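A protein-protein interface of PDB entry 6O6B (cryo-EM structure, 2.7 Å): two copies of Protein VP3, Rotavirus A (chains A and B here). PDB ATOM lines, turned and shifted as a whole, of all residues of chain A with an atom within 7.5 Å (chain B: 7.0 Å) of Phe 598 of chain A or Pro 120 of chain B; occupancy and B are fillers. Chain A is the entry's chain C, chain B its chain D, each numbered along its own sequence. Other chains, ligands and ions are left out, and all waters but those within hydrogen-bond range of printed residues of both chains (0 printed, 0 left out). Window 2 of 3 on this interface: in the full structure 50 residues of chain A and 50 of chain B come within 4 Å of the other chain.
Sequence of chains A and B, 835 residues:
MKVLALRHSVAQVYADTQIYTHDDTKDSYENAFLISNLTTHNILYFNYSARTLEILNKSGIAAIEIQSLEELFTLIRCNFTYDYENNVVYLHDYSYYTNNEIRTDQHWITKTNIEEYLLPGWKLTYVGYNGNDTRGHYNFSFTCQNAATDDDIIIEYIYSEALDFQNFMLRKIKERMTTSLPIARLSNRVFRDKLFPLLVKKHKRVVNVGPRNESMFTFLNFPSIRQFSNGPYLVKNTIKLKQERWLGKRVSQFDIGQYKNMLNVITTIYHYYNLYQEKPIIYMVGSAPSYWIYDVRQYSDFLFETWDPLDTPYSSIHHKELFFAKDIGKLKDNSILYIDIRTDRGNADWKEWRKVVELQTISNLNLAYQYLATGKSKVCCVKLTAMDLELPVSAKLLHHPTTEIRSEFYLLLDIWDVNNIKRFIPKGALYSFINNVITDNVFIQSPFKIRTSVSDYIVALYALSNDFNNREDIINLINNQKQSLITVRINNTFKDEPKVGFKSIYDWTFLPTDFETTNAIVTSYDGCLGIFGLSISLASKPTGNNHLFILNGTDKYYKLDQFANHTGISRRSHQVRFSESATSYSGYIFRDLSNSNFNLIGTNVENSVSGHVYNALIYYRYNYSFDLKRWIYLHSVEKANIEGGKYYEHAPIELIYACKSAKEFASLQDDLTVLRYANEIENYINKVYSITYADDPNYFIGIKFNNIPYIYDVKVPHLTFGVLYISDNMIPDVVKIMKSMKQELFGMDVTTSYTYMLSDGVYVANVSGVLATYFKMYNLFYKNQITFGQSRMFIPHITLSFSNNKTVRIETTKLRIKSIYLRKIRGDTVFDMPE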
ATOM      1  N   ILE A 589      17.457 -11.454  -4.753  1.00  0.00           N
ATOM      2  CA  ILE A 589      18.724 -11.277  -4.054  1.00  0.00           C
ATOM      3  C   ILE A 589      18.641 -10.079  -3.118  1.00  0.00           C
ATOM      4  O   ILE A 589      19.136 -10.125  -1.988  1.00  0.00           O
ATOM      5  CB  ILE A 589      19.882 -11.131  -5.060  1.00  0.00           C
ATOM      6  CG1 ILE A 589      20.057 -12.430  -5.854  1.00  0.00           C
ATOM      7  CG2 ILE A 589      21.186 -10.822  -4.344  1.00  0.00           C
ATOM      8  CD1 ILE A 589      20.922 -12.339  -7.100  1.00  0.00           C
ATOM      9  N   ARG A 591      16.222  -8.490  -1.454  1.00  0.00           N
ATOM     10  CA  ARG A 591      15.417  -8.460  -0.244  1.00  0.00           C
ATOM     11  C   ARG A 591      16.002  -9.357   0.834  1.00  0.00           C
ATOM     12  O   ARG A 591      15.761  -9.137   2.025  1.00  0.00           O
ATOM     13  CB  ARG A 591      13.979  -8.837  -0.566  1.00  0.00           C
ATOM     14  CG  ARG A 591      13.747 -10.235  -1.055  1.00  0.00           C
ATOM     15  CD  ARG A 591      12.268 -10.466  -1.240  1.00  0.00           C
ATOM     16  NE  ARG A 591      11.700  -9.592  -2.266  1.00  0.00           N
ATOM     17  CZ  ARG A 591      11.626  -9.891  -3.557  1.00  0.00           C
ATOM     18  NH1 ARG A 591      12.088 -11.028  -4.026  1.00  0.00           N
ATOM     19  NH2 ARG A 591      11.102  -9.039  -4.409  1.00  0.00           N
ATOM     20  N   ASP A 592      16.781 -10.363   0.449  1.00  0.00           N
ATOM     21  CA  ASP A 592      17.475 -11.163   1.451  1.00  0.00           C
ATOM     22  C   ASP A 592      18.693 -10.430   1.998  1.00  0.00           C
ATOM     23  O   ASP A 592      18.997 -10.531   3.191  1.00  0.00           O
ATOM     24  CB  ASP A 592      17.880 -12.512   0.864  1.00  0.00           C
ATOM     25  CG  ASP A 592      16.687 -13.422   0.618  1.00  0.00           C
ATOM     26  OD1 ASP A 592      15.702 -13.340   1.380  1.00  0.00           O
ATOM     27  OD2 ASP A 592      16.728 -14.215  -0.345  1.00  0.00           O
ATOM     28  N   LEU A 593      19.400  -9.690   1.144  1.00  0.00           N
ATOM     29  CA  LEU A 593      20.514  -8.883   1.619  1.00  0.00           C
ATOM     30  C   LEU A 593      20.036  -7.811   2.582  1.00  0.00           C
ATOM     31  O   LEU A 593      20.684  -7.538   3.597  1.00  0.00           O
ATOM     32  CB  LEU A 593      21.232  -8.231   0.445  1.00  0.00           C
ATOM     33  CG  LEU A 593      21.953  -9.079  -0.587  1.00  0.00           C
ATOM     34  CD1 LEU A 593      22.426  -8.187  -1.652  1.00  0.00           C
ATOM     35  CD2 LEU A 593      23.128  -9.782  -0.011  1.00  0.00           C
ATOM     36  N   SER A 594      18.909  -7.182   2.271  1.00  0.00           N
ATOM     37  CA  SER A 594      18.394  -6.097   3.087  1.00  0.00           C
ATOM     38  C   SER A 594      17.679  -6.574   4.340  1.00  0.00           C
ATOM     39  O   SER A 594      17.242  -5.734   5.131  1.00  0.00           O
ATOM     40  CB  SER A 594      17.445  -5.245   2.257  1.00  0.00           C
ATOM     41  OG  SER A 594      16.269  -5.966   1.960  1.00  0.00           O
ATOM     42  N   ASN A 595      17.526  -7.884   4.523  1.00  0.00           N
ATOM     43  CA  ASN A 595      16.963  -8.459   5.737  1.00  0.00           C
ATOM     44  C   ASN A 595      17.928  -9.431   6.409  1.00  0.00           C
ATOM     45  O   ASN A 595      17.497 -10.333   7.132  1.00  0.00           O
ATOM     46  CB  ASN A 595      15.633  -9.135   5.421  1.00  0.00           C
ATOM     47  CG  ASN A 595      14.585  -8.154   4.958  1.00  0.00           C
ATOM     48  OD1 ASN A 595      14.109  -8.220   3.832  1.00  0.00           O
ATOM     49  ND2 ASN A 595      14.225  -7.228   5.829  1.00  0.00           N
ATOM     50  N   SER A 596      19.228  -9.254   6.180  1.00  0.00           N
ATOM     51  CA  SER A 596      20.283  -9.954   6.907  1.00  0.00           C
ATOM     52  C   SER A 596      20.201 -11.466   6.725  1.00  0.00           C
ATOM     53  O   SER A 596      20.399 -12.237   7.665  1.00  0.00           O
ATOM     54  CB  SER A 596      20.269  -9.581   8.386  1.00  0.00           C
ATOM     55  OG  SER A 596      20.495  -8.187   8.532  1.00  0.00           O
ATOM     56  N   ASN A 597      19.912 -11.886   5.501  1.00  0.00           N
ATOM     57  CA  ASN A 597      20.166 -13.239   5.035  1.00  0.00           C
ATOM     58  C   ASN A 597      21.138 -13.155   3.880  1.00  0.00           C
ATOM     59  O   ASN A 597      20.973 -13.783   2.833  1.00  0.00           O
ATOM     60  CB  ASN A 597      18.890 -13.963   4.615  1.00  0.00           C
ATOM     61  CG  ASN A 597      19.126 -15.447   4.356  1.00  0.00           C
ATOM     62  OD1 ASN A 597      20.211 -15.969   4.614  1.00  0.00           O
ATOM     63  ND2 ASN A 597      18.139 -16.112   3.785  1.00  0.00           N
ATOM     64  N   PHE A 598      22.153 -12.334   4.064  1.00  0.00           N
ATOM     65  CA  PHE A 598      23.051 -11.982   2.984  1.00  0.00           C
ATOM     66  C   PHE A 598      24.104 -13.045   2.741  1.00  0.00           C
ATOM     67  O   PHE A 598      24.654 -13.115   1.637  1.00  0.00           O
ATOM     68  CB  PHE A 598      23.712 -10.623   3.268  1.00  0.00           C
ATOM     69  CG  PHE A 598      24.502 -10.584   4.533  1.00  0.00           C
ATOM     70  CD1 PHE A 598      23.938 -10.123   5.702  1.00  0.00           C
ATOM     71  CD2 PHE A 598      25.801 -11.015   4.560  1.00  0.00           C
ATOM     72  CE1 PHE A 598      24.670 -10.099   6.867  1.00  0.00           C
ATOM     73  CE2 PHE A 598      26.516 -10.994   5.712  1.00  0.00           C
ATOM     74  CZ  PHE A 598      25.964 -10.535   6.863  1.00  0.00           C
ATOM     75  N   ASN A 599      24.391 -13.869   3.738  1.00  0.00           N
ATOM     76  CA  ASN A 599      25.261 -15.007   3.502  1.00  0.00           C
ATOM     77  C   ASN A 599      24.674 -15.950   2.462  1.00  0.00           C
ATOM     78  O   ASN A 599      25.421 -16.538   1.673  1.00  0.00           O
ATOM     79  CB  ASN A 599      25.545 -15.746   4.811  1.00  0.00           C
ATOM     80  CG  ASN A 599      24.286 -16.158   5.549  1.00  0.00           C
ATOM     81  OD1 ASN A 599      23.170 -15.914   5.087  1.00  0.00           O
ATOM     82  ND2 ASN A 599      24.462 -16.815   6.696  1.00  0.00           N
ATOM     83  N   LEU A 600      23.346 -16.100   2.438  1.00  0.00           N
ATOM     84  CA  LEU A 600      22.689 -17.109   1.612  1.00  0.00           C
ATOM     85  C   LEU A 600      21.694 -16.435   0.684  1.00  0.00           C
ATOM     86  O   LEU A 600      20.706 -15.854   1.139  1.00  0.00           O
ATOM     87  CB  LEU A 600      21.981 -18.160   2.462  1.00  0.00           C
ATOM     88  CG  LEU A 600      22.789 -19.365   2.950  1.00  0.00           C
ATOM     89  CD1 LEU A 600      23.370 -20.246   1.853  1.00  0.00           C
ATOM     90  CD2 LEU A 600      23.815 -19.017   3.972  1.00  0.00           C
ATOM     91  N   ILE A 601      21.970 -16.518  -0.611  1.00  0.00           N
ATOM     92  CA  ILE A 601      21.014 -16.149  -1.638  1.00  0.00           C
ATOM     93  C   ILE A 601      20.931 -17.268  -2.667  1.00  0.00           C
ATOM     94  O   ILE A 601      20.645 -17.022  -3.842  1.00  0.00           O
ATOM     95  CB  ILE A 601      21.398 -14.804  -2.271  1.00  0.00           C
ATOM     96  CG1 ILE A 601      22.819 -14.849  -2.812  1.00  0.00           C
ATOM     97  CG2 ILE A 601      21.291 -13.718  -1.247  1.00  0.00           C
ATOM     98  CD1 ILE A 601      23.151 -13.692  -3.657  1.00  0.00           C
ATOM     99  N   GLY A 602      21.213 -18.499  -2.240  1.00  0.00           N
ATOM    100  CA  GLY A 602      21.022 -19.651  -3.093  1.00  0.00           C
ATOM    101  C   GLY A 602      19.574 -20.063  -3.141  1.00  0.00           C
ATOM    102  O   GLY A 602      19.022 -20.318  -4.215  1.00  0.00           O
ATOM    103  N   TYR A 756      26.655 -24.547   4.937  1.00  0.00           N
ATOM    104  CA  TYR A 756      27.036 -23.157   4.761  1.00  0.00           C
ATOM    105  C   TYR A 756      27.565 -22.604   6.072  1.00  0.00           C
ATOM    106  O   TYR A 756      27.619 -23.292   7.093  1.00  0.00           O
ATOM    107  CB  TYR A 756      25.869 -22.313   4.245  1.00  0.00           C
ATOM    108  CG  TYR A 756      24.661 -22.190   5.152  1.00  0.00           C
ATOM    109  CD1 TYR A 756      23.558 -23.004   4.984  1.00  0.00           C
ATOM    110  CD2 TYR A 756      24.619 -21.239   6.162  1.00  0.00           C
ATOM    111  CE1 TYR A 756      22.446 -22.869   5.796  1.00  0.00           C
ATOM    112  CE2 TYR A 756      23.516 -21.085   6.953  1.00  0.00           C
ATOM    113  CZ  TYR A 756      22.437 -21.911   6.780  1.00  0.00           C
ATOM    114  OH  TYR A 756      21.353 -21.756   7.608  1.00  0.00           O
ATOM    115  N   MET A 757      27.961 -21.338   6.012  1.00  0.00           N
ATOM    116  CA  MET A 757      28.395 -20.588   7.176  1.00  0.00           C
ATOM    117  C   MET A 757      27.296 -19.620   7.576  1.00  0.00           C
ATOM    118  O   MET A 757      27.046 -18.631   6.880  1.00  0.00           O
ATOM    119  CB  MET A 757      29.676 -19.826   6.861  1.00  0.00           C
ATOM    120  CG  MET A 757      30.884 -20.704   6.583  1.00  0.00           C
ATOM    121  SD  MET A 757      31.326 -21.820   7.922  1.00  0.00           S
ATOM    122  CE  MET A 757      31.776 -20.677   9.205  1.00  0.00           C
ATOM    123  N   LEU A 758      26.631 -19.908   8.689  1.00  0.00           N
ATOM    124  CA  LEU A 758      25.636 -18.990   9.218  1.00  0.00           C
ATOM    125  C   LEU A 758      26.303 -17.779   9.842  1.00  0.00           C
ATOM    126  O   LEU A 758      25.765 -16.668   9.792  1.00  0.00           O
ATOM    127  CB  LEU A 758      24.763 -19.692  10.261  1.00  0.00           C
ATOM    128  CG  LEU A 758      23.601 -18.888  10.847  1.00  0.00           C
ATOM    129  CD1 LEU A 758      22.567 -18.554   9.769  1.00  0.00           C
ATOM    130  CD2 LEU A 758      22.956 -19.626  11.994  1.00  0.00           C
ATOM    131  N   SER A 759      27.474 -17.994  10.423  1.00  0.00           N
ATOM    132  CA  SER A 759      28.225 -16.966  11.114  1.00  0.00           C
ATOM    133  C   SER A 759      29.597 -17.539  11.421  1.00  0.00           C
ATOM    134  O   SER A 759      29.888 -18.695  11.109  1.00  0.00           O
ATOM    135  CB  SER A 759      27.503 -16.524  12.383  1.00  0.00           C
ATOM    136  OG  SER A 759      27.442 -17.565  13.341  1.00  0.00           O
ATOM    137  N   ASP A 760      30.444 -16.726  12.041  1.00  0.00           N
ATOM    138  CA  ASP A 760      31.747 -17.213  12.459  1.00  0.00           C
ATOM    139  C   ASP A 760      31.590 -18.341  13.467  1.00  0.00           C
ATOM    140  O   ASP A 760      30.759 -18.268  14.378  1.00  0.00           O
ATOM    141  CB  ASP A 760      32.575 -16.084  13.064  1.00  0.00           C
ATOM    142  CG  ASP A 760      33.951 -16.544  13.492  1.00  0.00           C
ATOM    143  OD1 ASP A 760      34.796 -16.801  12.609  1.00  0.00           O
ATOM    144  OD2 ASP A 760      34.187 -16.652  14.712  1.00  0.00           O
ATOM    145  N   ILE A 795      16.115 -18.270   9.675  1.00  0.00           N
ATOM    146  CA  ILE A 795      16.603 -19.137   8.609  1.00  0.00           C
ATOM    147  C   ILE A 795      16.799 -20.514   9.235  1.00  0.00           C
ATOM    148  O   ILE A 795      17.712 -20.677  10.057  1.00  0.00           O
ATOM    149  CB  ILE A 795      17.898 -18.582   7.988  1.00  0.00           C
ATOM    150  CG1 ILE A 795      17.674 -17.173   7.427  1.00  0.00           C
ATOM    151  CG2 ILE A 795      18.429 -19.487   6.886  1.00  0.00           C
ATOM    152  CD1 ILE A 795      16.597 -17.055   6.337  1.00  0.00           C
ATOM    153  N   ASN A 804      35.115 -23.197  10.908  1.00  0.00           N
ATOM    154  CA  ASN A 804      34.906 -22.456   9.671  1.00  0.00           C
ATOM    155  C   ASN A 804      35.375 -23.342   8.524  1.00  0.00           C
ATOM    156  O   ASN A 804      36.578 -23.585   8.378  1.00  0.00           O
ATOM    157  CB  ASN A 804      35.659 -21.126   9.688  1.00  0.00           C
ATOM    158  CG  ASN A 804      35.159 -20.179  10.764  1.00  0.00           C
ATOM    159  OD1 ASN A 804      33.967 -20.116  11.050  1.00  0.00           O
ATOM    160  ND2 ASN A 804      36.072 -19.420  11.351  1.00  0.00           N
ATOM    161  N   ASN B 100      26.661 -18.108  -4.179  1.00  0.00           N
ATOM    162  CA  ASN B 100      27.399 -17.417  -3.121  1.00  0.00           C
ATOM    163  C   ASN B 100      28.889 -17.363  -3.404  1.00  0.00           C
ATOM    164  O   ASN B 100      29.713 -17.917  -2.677  1.00  0.00           O
ATOM    165  CB  ASN B 100      27.127 -18.029  -1.755  1.00  0.00           C
ATOM    166  CG  ASN B 100      25.752 -17.704  -1.260  1.00  0.00           C
ATOM    167  OD1 ASN B 100      25.280 -16.575  -1.378  1.00  0.00           O
ATOM    168  ND2 ASN B 100      25.089 -18.689  -0.726  1.00  0.00           N
ATOM    169  N   GLU B 115      39.479 -13.985   1.663  1.00  0.00           N
ATOM    170  CA  GLU B 115      38.330 -14.792   2.051  1.00  0.00           C
ATOM    171  C   GLU B 115      38.064 -14.708   3.551  1.00  0.00           C
ATOM    172  O   GLU B 115      36.966 -15.049   4.002  1.00  0.00           O
ATOM    173  CB  GLU B 115      38.528 -16.242   1.597  1.00  0.00           C
ATOM    174  CG  GLU B 115      39.645 -17.040   2.296  1.00  0.00           C
ATOM    175  CD  GLU B 115      41.016 -16.818   1.694  1.00  0.00           C
ATOM    176  OE1 GLU B 115      41.180 -15.867   0.900  1.00  0.00           O
ATOM    177  OE2 GLU B 115      41.937 -17.587   2.036  1.00  0.00           O
ATOM    178  N   TYR B 117      37.859 -11.826   4.685  1.00  0.00           N
ATOM    179  CA  TYR B 117      37.275 -10.493   4.688  1.00  0.00           C
ATOM    180  C   TYR B 117      36.014 -10.411   3.838  1.00  0.00           C
ATOM    181  O   TYR B 117      35.335  -9.380   3.852  1.00  0.00           O
ATOM    182  CB  TYR B 117      38.326  -9.477   4.218  1.00  0.00           C
ATOM    183  CG  TYR B 117      39.568  -9.365   5.107  1.00  0.00           C
ATOM    184  CD1 TYR B 117      39.568  -9.821   6.410  1.00  0.00           C
ATOM    185  CD2 TYR B 117      40.741  -8.814   4.630  1.00  0.00           C
ATOM    186  CE1 TYR B 117      40.669  -9.733   7.212  1.00  0.00           C
ATOM    187  CE2 TYR B 117      41.866  -8.726   5.432  1.00  0.00           C
ATOM    188  CZ  TYR B 117      41.816  -9.184   6.725  1.00  0.00           C
ATOM    189  OH  TYR B 117      42.913  -9.100   7.542  1.00  0.00           O
ATOM    190  N   LEU B 118      35.668 -11.470   3.118  1.00  0.00           N
ATOM    191  CA  LEU B 118      34.367 -11.566   2.485  1.00  0.00           C
ATOM    192  C   LEU B 118      33.293 -11.829   3.534  1.00  0.00           C
ATOM    193  O   LEU B 118      33.571 -12.230   4.666  1.00  0.00           O
ATOM    194  CB  LEU B 118      34.338 -12.683   1.445  1.00  0.00           C
ATOM    195  CG  LEU B 118      35.184 -12.592   0.181  1.00  0.00           C
ATOM    196  CD1 LEU B 118      35.169 -13.887  -0.584  1.00  0.00           C
ATOM    197  CD2 LEU B 118      34.637 -11.534  -0.688  1.00  0.00           C
ATOM    198  N   LEU B 119      32.050 -11.590   3.136  1.00  0.00           N
ATOM    199  CA  LEU B 119      30.911 -11.934   3.966  1.00  0.00           C
ATOM    200  C   LEU B 119      30.938 -13.436   4.271  1.00  0.00           C
ATOM    201  O   LEU B 119      31.493 -14.217   3.493  1.00  0.00           O
ATOM    202  CB  LEU B 119      29.623 -11.538   3.239  1.00  0.00           C
ATOM    203  CG  LEU B 119      29.412 -10.067   2.882  1.00  0.00           C
ATOM    204  CD1 LEU B 119      28.198  -9.930   1.993  1.00  0.00           C
ATOM    205  CD2 LEU B 119      29.283  -9.157   4.097  1.00  0.00           C
ATOM    206  N   PRO B 120      30.365 -13.875   5.399  1.00  0.00           N
ATOM    207  CA  PRO B 120      30.505 -15.278   5.807  1.00  0.00           C
ATOM    208  C   PRO B 120      29.809 -16.246   4.866  1.00  0.00           C
ATOM    209  O   PRO B 120      28.583 -16.229   4.729  1.00  0.00           O
ATOM    210  CB  PRO B 120      29.849 -15.304   7.187  1.00  0.00           C
ATOM    211  CG  PRO B 120      28.875 -14.210   7.144  1.00  0.00           C
ATOM    212  CD  PRO B 120      29.481 -13.146   6.318  1.00  0.00           C
ATOM    213  N   GLY B 121      30.604 -17.101   4.227  1.00  0.00           N
ATOM    214  CA  GLY B 121      30.101 -18.143   3.364  1.00  0.00           C
ATOM    215  C   GLY B 121      30.471 -17.972   1.910  1.00  0.00           C
ATOM    216  O   GLY B 121      30.312 -18.905   1.121  1.00  0.00           O
ATOM    217  N   TRP B 122      30.966 -16.803   1.543  1.00  0.00           N
ATOM    218  CA  TRP B 122      31.241 -16.459   0.165  1.00  0.00           C
ATOM    219  C   TRP B 122      32.665 -16.854  -0.193  1.00  0.00           C
ATOM    220  O   TRP B 122      33.498 -17.113   0.679  1.00  0.00           O
ATOM    221  CB  TRP B 122      31.025 -14.964  -0.032  1.00  0.00           C
ATOM    222  CG  TRP B 122      29.620 -14.563   0.126  1.00  0.00           C
ATOM    223  CD1 TRP B 122      28.963 -14.387   1.300  1.00  0.00           C
ATOM    224  CD2 TRP B 122      28.699 -14.202  -0.907  1.00  0.00           C
ATOM    225  NE1 TRP B 122      27.675 -13.974   1.062  1.00  0.00           N
ATOM    226  CE2 TRP B 122      27.493 -13.852  -0.286  1.00  0.00           C
ATOM    227  CE3 TRP B 122      28.772 -14.159  -2.290  1.00  0.00           C
ATOM    228  CZ2 TRP B 122      26.377 -13.467  -0.996  1.00  0.00           C
ATOM    229  CZ3 TRP B 122      27.661 -13.775  -2.993  1.00  0.00           C
ATOM    230  CH2 TRP B 122      26.479 -13.436  -2.347  1.00  0.00           C
ATOM    231  N   GLN B 166      33.531  -5.744   4.043  1.00  0.00           N
ATOM    232  CA  GLN B 166      32.187  -6.310   4.069  1.00  0.00           C
ATOM    233  C   GLN B 166      31.142  -5.232   3.865  1.00  0.00           C
ATOM    234  O   GLN B 166      30.169  -5.422   3.128  1.00  0.00           O
ATOM    235  CB  GLN B 166      31.952  -7.021   5.392  1.00  0.00           C
ATOM    236  CG  GLN B 166      32.810  -8.239   5.582  1.00  0.00           C
ATOM    237  CD  GLN B 166      32.510  -8.964   6.878  1.00  0.00           C
ATOM    238  OE1 GLN B 166      31.626  -8.569   7.636  1.00  0.00           O
ATOM    239  NE2 GLN B 166      33.260 -10.017   7.147  1.00  0.00           N
ATOM    240  N   LEU B 170      28.951  -5.384   0.251  1.00  0.00           N
ATOM    241  CA  LEU B 170      27.519  -5.420   0.502  1.00  0.00           C
ATOM    242  C   LEU B 170      26.830  -4.199  -0.080  1.00  0.00           C
ATOM    243  O   LEU B 170      25.680  -4.277  -0.515  1.00  0.00           O
ATOM    244  CB  LEU B 170      27.257  -5.527   1.993  1.00  0.00           C
ATOM    245  CG  LEU B 170      25.806  -5.614   2.456  1.00  0.00           C
ATOM    246  CD1 LEU B 170      25.175  -6.849   1.919  1.00  0.00           C
ATOM    247  CD2 LEU B 170      25.713  -5.606   3.971  1.00  0.00           C
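OD1 of Asn 597 of chain A lies close to OD1 of Asn 599 of chain A. The side-chain amide nitrogen (ND2) of Asn 599 of chain A is in hydrogen-bond range of the backbone carbonyl oxygen (O) of Met 757 of chain A (3.2 Å). O of Leu 758 of chain A sits at hydrogen-bond distance from ND2 of Asn 599 of chain A, at 3.4 Å.
NE1 of Trp 122 of chain B sits close to O of Phe 598 of chain A, at 3.2 Å. O of Asn 599 of chain A sits close to OD1 of Asn 100 of chain B, 3.1 Å away. The backbone carbonyl oxygen of Asn 599 of chain A is in hydrogen-bond range of the indole nitrogen of Trp 122 of chain B (3.5 Å). The backbone NH (N) of Ile 601 of chain A lies close to the side-chain amide oxygen (OD1) of Asn 100 of chain B, at 3.4 Å.
Printed residues of chain B within 4 Å of Phe 598 of chain A: Leu 119 (3.7 Å), Pro 120 (3.7 Å) and Trp 122 (3.2 Å). Printed residues of chain B within 4 Å of Asn 599 of chain A: Asn 100 (3.1 Å), Pro 120 (3.1 Å) and Trp 122 (3.5 Å). Printed residues of chain B within 4 Å of Met 757 of chain A: Pro 120 and Gly 121. Of the printed residues of chain A, Asn 100 of chain B touches Asn 599, Leu 600 and Ile 601. Of the printed residues of chain A, Pro 120 of chain B touches Phe 598, Asn 599 and Met 757. Of the printed residues of chain A, Trp 122 of chain B touches Phe 598, Asn 599 and Ile 601. The nearest printed residue of chain A that does not touch Gly 121 of chain B is Asn 599 of chain A (5.2 Å).
Hydrophobic or aromatic side chains of chain B that line the printed part of chain A: Leu 119, Pro 120 and Trp 122. Printed residues of chain A that touch a printed residue of chain B: Phe 598, Asn 599, Leu 600, Ile 601 and Met 757. Along chain A the printed residues that touch a printed residue of chain B span positions 598 to 757. Among the printed residues, no Asp or Glu carboxylate lies within 4 Å of a Lys or Arg side-chain nitrogen of the other chain.
No position is printed for both chains. Of the 11 pairs that touch across the chains among the printed residues, none has its exchanged pair printed and touching as well.
Among the printed residues, pairs that only touch across the chains: Asn 599 of chain A with Pro 120 of chain B (3.1 Å), Leu 600 of chain A with Asn 100 of chain B (3.5 Å), Met 757 of chain A with Pro 120 of chain B (3.6 Å), Ile 601 of chain A with Trp 122 of chain B (3.6 Å), Phe 598 of chain A with Leu 119 of chain B (3.7 Å), Phe 598 of chain A with Pro 120 of chain B (3.7 Å) and Met 757 of chain A with Gly 121 of chain B (3.9 Å).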
